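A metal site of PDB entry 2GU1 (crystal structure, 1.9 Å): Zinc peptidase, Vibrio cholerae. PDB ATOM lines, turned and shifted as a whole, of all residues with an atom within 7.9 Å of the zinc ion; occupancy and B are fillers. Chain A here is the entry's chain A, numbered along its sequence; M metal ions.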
ATOM      1  N   LEU A  40      30.050   3.239  10.547  1.00  0.00           N
ATOM      2  CA  LEU A  40      30.237   1.850  10.953  1.00  0.00           C
ATOM      3  C   LEU A  40      29.337   0.940  10.116  1.00  0.00           C
ATOM      4  O   LEU A  40      29.752  -0.121   9.671  1.00  0.00           O
ATOM      5  CB  LEU A  40      29.876   1.672  12.437  1.00  0.00           C
ATOM      6  CG  LEU A  40      29.598   0.249  12.953  1.00  0.00           C
ATOM      7  CD1 LEU A  40      30.812  -0.631  12.754  1.00  0.00           C
ATOM      8  CD2 LEU A  40      29.217   0.315  14.434  1.00  0.00           C
ATOM      9  N   ASP A  41      28.113   1.376   9.888  1.00  0.00           N
ATOM     10  CA  ASP A  41      27.144   0.599   9.133  1.00  0.00           C
ATOM     11  C   ASP A  41      27.218   0.696   7.612  1.00  0.00           C
ATOM     12  O   ASP A  41      26.407   0.082   6.908  1.00  0.00           O
ATOM     13  CB  ASP A  41      25.746   0.974   9.599  1.00  0.00           C
ATOM     14  CG  ASP A  41      25.531   0.682  11.061  1.00  0.00           C
ATOM     15  OD1 ASP A  41      25.690  -0.495  11.437  1.00  0.00           O
ATOM     16  OD2 ASP A  41      25.239   1.614  11.835  1.00  0.00           O
ATOM     17  N   THR A 214      22.222 -13.692  16.141  1.00  0.00           N
ATOM     18  CA  THR A 214      21.704 -12.859  17.223  1.00  0.00           C
ATOM     19  C   THR A 214      21.050 -11.576  16.720  1.00  0.00           C
ATOM     20  O   THR A 214      20.376 -10.878  17.471  1.00  0.00           O
ATOM     21  CB  THR A 214      22.834 -12.493  18.220  1.00  0.00           C
ATOM     22  OG1 THR A 214      23.886 -11.800  17.529  1.00  0.00           O
ATOM     23  CG2 THR A 214      23.399 -13.749  18.862  1.00  0.00           C
ATOM     24  N   SER A 215      21.248 -11.287  15.431  1.00  0.00           N
ATOM     25  CA  SER A 215      20.676 -10.104  14.796  1.00  0.00           C
ATOM     26  C   SER A 215      20.893 -10.205  13.288  1.00  0.00           C
ATOM     27  O   SER A 215      22.027 -10.203  12.822  1.00  0.00           O
ATOM     28  CB  SER A 215      21.364  -8.844  15.327  1.00  0.00           C
ATOM     29  OG  SER A 215      20.874  -7.689  14.665  1.00  0.00           O
ATOM     30  N   GLY A 216      19.802 -10.298  12.541  1.00  0.00           N
ATOM     31  CA  GLY A 216      19.900 -10.426  11.102  1.00  0.00           C
ATOM     32  C   GLY A 216      19.911  -9.128  10.328  1.00  0.00           C
ATOM     33  O   GLY A 216      19.847  -8.042  10.900  1.00  0.00           O
ATOM     34  N   PHE A 217      19.970  -9.253   9.002  1.00  0.00           N
ATOM     35  CA  PHE A 217      19.978  -8.117   8.079  1.00  0.00           C
ATOM     36  C   PHE A 217      18.659  -7.352   8.182  1.00  0.00           C
ATOM     37  O   PHE A 217      17.599  -7.968   8.174  1.00  0.00           O
ATOM     38  CB  PHE A 217      20.160  -8.629   6.645  1.00  0.00           C
ATOM     39  CG  PHE A 217      20.259  -7.549   5.599  1.00  0.00           C
ATOM     40  CD1 PHE A 217      21.471  -6.910   5.361  1.00  0.00           C
ATOM     41  CD2 PHE A 217      19.160  -7.217   4.810  1.00  0.00           C
ATOM     42  CE1 PHE A 217      21.596  -5.948   4.353  1.00  0.00           C
ATOM     43  CE2 PHE A 217      19.272  -6.259   3.798  1.00  0.00           C
ATOM     44  CZ  PHE A 217      20.488  -5.619   3.574  1.00  0.00           C
ATOM     45  N   ARG A 221      15.874  -0.942  10.082  1.00  0.00           N
ATOM     46  CA  ARG A 221      15.992  -0.893  11.543  1.00  0.00           C
ATOM     47  C   ARG A 221      15.977   0.556  12.054  1.00  0.00           C
ATOM     48  O   ARG A 221      16.622   1.431  11.480  1.00  0.00           O
ATOM     49  CB  ARG A 221      17.284  -1.578  11.991  1.00  0.00           C
ATOM     50  CG  ARG A 221      17.440  -1.650  13.501  1.00  0.00           C
ATOM     51  CD  ARG A 221      18.802  -2.176  13.912  1.00  0.00           C
ATOM     52  NE  ARG A 221      19.879  -1.364  13.353  1.00  0.00           N
ATOM     53  CZ  ARG A 221      21.173  -1.515  13.654  1.00  0.00           C
ATOM     54  NH1 ARG A 221      21.552  -2.440  14.520  1.00  0.00           N
ATOM     55  NH2 ARG A 221      22.075  -0.738  13.078  1.00  0.00           N
ATOM     56  N   PRO A 231      20.201   1.325   9.507  1.00  0.00           N
ATOM     57  CA  PRO A 231      20.260  -0.035   8.978  1.00  0.00           C
ATOM     58  C   PRO A 231      21.332  -0.956   9.529  1.00  0.00           C
ATOM     59  O   PRO A 231      22.463  -0.541   9.819  1.00  0.00           O
ATOM     60  CB  PRO A 231      20.435   0.187   7.473  1.00  0.00           C
ATOM     61  CG  PRO A 231      21.290   1.425   7.434  1.00  0.00           C
ATOM     62  CD  PRO A 231      20.620   2.310   8.479  1.00  0.00           C
ATOM     63  N   HIS A 232      20.964  -2.219   9.706  1.00  0.00           N
ATOM     64  CA  HIS A 232      21.904  -3.232  10.137  1.00  0.00           C
ATOM     65  C   HIS A 232      22.142  -3.931   8.804  1.00  0.00           C
ATOM     66  O   HIS A 232      21.313  -4.726   8.351  1.00  0.00           O
ATOM     67  CB  HIS A 232      21.295  -4.203  11.133  1.00  0.00           C
ATOM     68  CG  HIS A 232      22.282  -5.192  11.676  1.00  0.00           C
ATOM     69  ND1 HIS A 232      22.068  -6.555  11.650  1.00  0.00           N
ATOM     70  CD2 HIS A 232      23.499  -5.016  12.245  1.00  0.00           C
ATOM     71  CE1 HIS A 232      23.100  -7.171  12.191  1.00  0.00           C
ATOM     72  NE2 HIS A 232      23.983  -6.251  12.555  1.00  0.00           N
ATOM     73  N   ASN A 233      23.268  -3.624   8.179  1.00  0.00           N
ATOM     74  CA  ASN A 233      23.611  -4.168   6.874  1.00  0.00           C
ATOM     75  C   ASN A 233      24.357  -5.503   6.866  1.00  0.00           C
ATOM     76  O   ASN A 233      25.059  -5.810   5.911  1.00  0.00           O
ATOM     77  CB  ASN A 233      24.400  -3.105   6.102  1.00  0.00           C
ATOM     78  CG  ASN A 233      23.523  -1.940   5.666  1.00  0.00           C
ATOM     79  OD1 ASN A 233      23.947  -0.788   5.687  1.00  0.00           O
ATOM     80  ND2 ASN A 233      22.300  -2.247   5.261  1.00  0.00           N
ATOM     81  N   GLY A 234      24.210  -6.285   7.933  1.00  0.00           N
ATOM     82  CA  GLY A 234      24.891  -7.565   7.974  1.00  0.00           C
ATOM     83  C   GLY A 234      24.184  -8.541   8.894  1.00  0.00           C
ATOM     84  O   GLY A 234      23.112  -8.261   9.405  1.00  0.00           O
ATOM     85  N   THR A 235      24.795  -9.706   9.093  1.00  0.00           N
ATOM     86  CA  THR A 235      24.225 -10.728   9.965  1.00  0.00           C
ATOM     87  C   THR A 235      25.175 -10.962  11.131  1.00  0.00           C
ATOM     88  O   THR A 235      26.377 -11.108  10.936  1.00  0.00           O
ATOM     89  CB  THR A 235      24.022 -12.052   9.202  1.00  0.00           C
ATOM     90  OG1 THR A 235      23.215 -11.819   8.035  1.00  0.00           O
ATOM     91  CG2 THR A 235      23.339 -13.076  10.075  1.00  0.00           C
ATOM     92  N   ASP A 236      24.647 -10.997  12.357  1.00  0.00           N
ATOM     93  CA  ASP A 236      25.476 -11.237  13.533  1.00  0.00           C
ATOM     94  C   ASP A 236      25.411 -12.680  14.002  1.00  0.00           C
ATOM     95  O   ASP A 236      24.314 -13.203  14.238  1.00  0.00           O
ATOM     96  CB  ASP A 236      25.046 -10.311  14.681  1.00  0.00           C
ATOM     97  CG  ASP A 236      25.272  -8.858  14.360  1.00  0.00           C
ATOM     98  OD1 ASP A 236      25.927  -8.583  13.341  1.00  0.00           O
ATOM     99  OD2 ASP A 236      24.803  -8.004  15.135  1.00  0.00           O
ATOM    100  N   PHE A 237      26.574 -13.327  14.115  1.00  0.00           N
ATOM    101  CA  PHE A 237      26.673 -14.720  14.574  1.00  0.00           C
ATOM    102  C   PHE A 237      27.217 -14.741  15.993  1.00  0.00           C
ATOM    103  O   PHE A 237      28.102 -13.945  16.350  1.00  0.00           O
ATOM    104  CB  PHE A 237      27.580 -15.529  13.644  1.00  0.00           C
ATOM    105  CG  PHE A 237      27.008 -15.758  12.272  1.00  0.00           C
ATOM    106  CD1 PHE A 237      25.891 -16.573  12.094  1.00  0.00           C
ATOM    107  CD2 PHE A 237      27.548 -15.119  11.155  1.00  0.00           C
ATOM    108  CE1 PHE A 237      25.330 -16.757  10.832  1.00  0.00           C
ATOM    109  CE2 PHE A 237      27.002 -15.294   9.889  1.00  0.00           C
ATOM    110  CZ  PHE A 237      25.893 -16.118   9.717  1.00  0.00           C
ATOM    111  N   LEU A 279      33.600  -8.047  10.351  1.00  0.00           N
ATOM    112  CA  LEU A 279      33.932  -7.017  11.343  1.00  0.00           C
ATOM    113  C   LEU A 279      34.100  -7.472  12.789  1.00  0.00           C
ATOM    114  O   LEU A 279      33.713  -8.578  13.172  1.00  0.00           O
ATOM    115  CB  LEU A 279      32.878  -5.922  11.317  1.00  0.00           C
ATOM    116  CG  LEU A 279      32.809  -4.955  10.133  1.00  0.00           C
ATOM    117  CD1 LEU A 279      32.634  -5.705   8.838  1.00  0.00           C
ATOM    118  CD2 LEU A 279      31.629  -3.989  10.376  1.00  0.00           C
ATOM    119  N   HIS A 280      34.698  -6.570  13.580  1.00  0.00           N
ATOM    120  CA  HIS A 280      34.946  -6.769  15.002  1.00  0.00           C
ATOM    121  C   HIS A 280      35.886  -7.925  15.311  1.00  0.00           C
ATOM    122  O   HIS A 280      35.909  -8.441  16.433  1.00  0.00           O
ATOM    123  CB  HIS A 280      33.614  -6.983  15.718  1.00  0.00           C
ATOM    124  CG  HIS A 280      32.603  -5.909  15.440  1.00  0.00           C
ATOM    125  ND1 HIS A 280      32.824  -4.577  15.745  1.00  0.00           N
ATOM    126  CD2 HIS A 280      31.381  -5.961  14.864  1.00  0.00           C
ATOM    127  CE1 HIS A 280      31.774  -3.864  15.378  1.00  0.00           C
ATOM    128  NE2 HIS A 280      30.883  -4.680  14.840  1.00  0.00           N
ATOM    129  N   HIS A 311      30.830 -10.699  18.904  1.00  0.00           N
ATOM    130  CA  HIS A 311      30.078 -11.343  17.842  1.00  0.00           C
ATOM    131  C   HIS A 311      30.729 -11.005  16.505  1.00  0.00           C
ATOM    132  O   HIS A 311      31.493 -10.051  16.392  1.00  0.00           O
ATOM    133  CB  HIS A 311      28.628 -10.835  17.800  1.00  0.00           C
ATOM    134  CG  HIS A 311      28.498  -9.403  17.368  1.00  0.00           C
ATOM    135  ND1 HIS A 311      28.852  -8.345  18.169  1.00  0.00           N
ATOM    136  CD2 HIS A 311      28.048  -8.853  16.210  1.00  0.00           C
ATOM    137  CE1 HIS A 311      28.615  -7.212  17.538  1.00  0.00           C
ATOM    138  NE2 HIS A 311      28.128  -7.497  16.344  1.00  0.00           N
ATOM    139  N   LEU A 312      30.412 -11.812  15.508  1.00  0.00           N
ATOM    140  CA  LEU A 312      30.926 -11.566  14.177  1.00  0.00           C
ATOM    141  C   LEU A 312      29.794 -10.880  13.415  1.00  0.00           C
ATOM    142  O   LEU A 312      28.641 -11.317  13.448  1.00  0.00           O
ATOM    143  CB  LEU A 312      31.276 -12.870  13.464  1.00  0.00           C
ATOM    144  CG  LEU A 312      31.662 -12.716  11.989  1.00  0.00           C
ATOM    145  CD1 LEU A 312      33.063 -12.120  11.873  1.00  0.00           C
ATOM    146  CD2 LEU A 312      31.619 -14.078  11.311  1.00  0.00           C
ATOM    147  N   HIS A 313      30.128  -9.772  12.753  1.00  0.00           N
ATOM    148  CA  HIS A 313      29.161  -9.058  11.939  1.00  0.00           C
ATOM    149  C   HIS A 313      29.616  -9.410  10.525  1.00  0.00           C
ATOM    150  O   HIS A 313      30.708  -9.014  10.115  1.00  0.00           O
ATOM    151  CB  HIS A 313      29.261  -7.555  12.175  1.00  0.00           C
ATOM    152  CG  HIS A 313      28.464  -6.730  11.221  1.00  0.00           C
ATOM    153  ND1 HIS A 313      27.197  -6.266  11.514  1.00  0.00           N
ATOM    154  CD2 HIS A 313      28.735  -6.311   9.963  1.00  0.00           C
ATOM    155  CE1 HIS A 313      26.729  -5.589  10.476  1.00  0.00           C
ATOM    156  NE2 HIS A 313      27.640  -5.608   9.520  1.00  0.00           N
ATOM    157  N   PHE A 314      28.784 -10.165   9.799  1.00  0.00           N
ATOM    158  CA  PHE A 314      29.111 -10.612   8.440  1.00  0.00           C
ATOM    159  C   PHE A 314      28.268  -9.894   7.388  1.00  0.00           C
ATOM    160  O   PHE A 314      27.055  -9.691   7.575  1.00  0.00           O
ATOM    161  CB  PHE A 314      28.880 -12.140   8.350  1.00  0.00           C
ATOM    162  CG  PHE A 314      29.100 -12.731   6.985  1.00  0.00           C
ATOM    163  CD1 PHE A 314      30.337 -12.665   6.362  1.00  0.00           C
ATOM    164  CD2 PHE A 314      28.048 -13.356   6.315  1.00  0.00           C
ATOM    165  CE1 PHE A 314      30.533 -13.231   5.089  1.00  0.00           C
ATOM    166  CE2 PHE A 314      28.226 -13.920   5.054  1.00  0.00           C
ATOM    167  CZ  PHE A 314      29.472 -13.858   4.430  1.00  0.00           C
ATOM    168  N   GLU A 315      28.896  -9.508   6.288  1.00  0.00           N
ATOM    169  CA  GLU A 315      28.184  -8.812   5.218  1.00  0.00           C
ATOM    170  C   GLU A 315      28.481  -9.379   3.852  1.00  0.00           C
ATOM    171  O   GLU A 315      29.586  -9.846   3.580  1.00  0.00           O
ATOM    172  CB  GLU A 315      28.546  -7.318   5.217  1.00  0.00           C
ATOM    173  CG  GLU A 315      27.845  -6.494   6.289  1.00  0.00           C
ATOM    174  CD  GLU A 315      28.214  -5.017   6.251  1.00  0.00           C
ATOM    175  OE1 GLU A 315      28.596  -4.510   5.171  1.00  0.00           O
ATOM    176  OE2 GLU A 315      28.116  -4.351   7.293  1.00  0.00           O
HETATM  177 ZN    ZN M   1      25.913  -6.570  13.074  1.00  0.00          ZN
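The backbone carbonyl oxygen of Gly 234 lies close to a ring nitrogen (ND1) of His 232 (3.0 Å).
OG of Ser 215 sits close to ND1 of His 232, at 3.4 Å.
O of Gly 216 sits at hydrogen-bond distance from ND1 of His 232 (2.8 Å).
O of Ser 215 sits at hydrogen-bond distance from N of Asp 236, 2.8 Å away.
The backbone carbonyl oxygen (O) of Asp 236 is in hydrogen-bond range of the backbone NH (N) of Thr 214 (2.9 Å).
OE2 of Glu 315 sits at hydrogen-bond distance from NE2 of His 313 (2.6 Å).
The backbone carbonyl oxygen of His 313 is in hydrogen-bond range of the backbone NH of Leu 279 (3.1 Å).
The zinc ion is bound by NE2 of His 232 (2.0 Å), OD1 of Asp 236 (2.0 Å) and ND1 of His 313 (2.0 Å).
Slightly farther from the zinc ion lies OD2 of Asp 236 (2.7 Å).
Of the 21 residues printed, 3 come within 4 Å of the zinc ion.
The nearest printed residue that does not touch the zinc ion is His 311 (4.1 Å).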
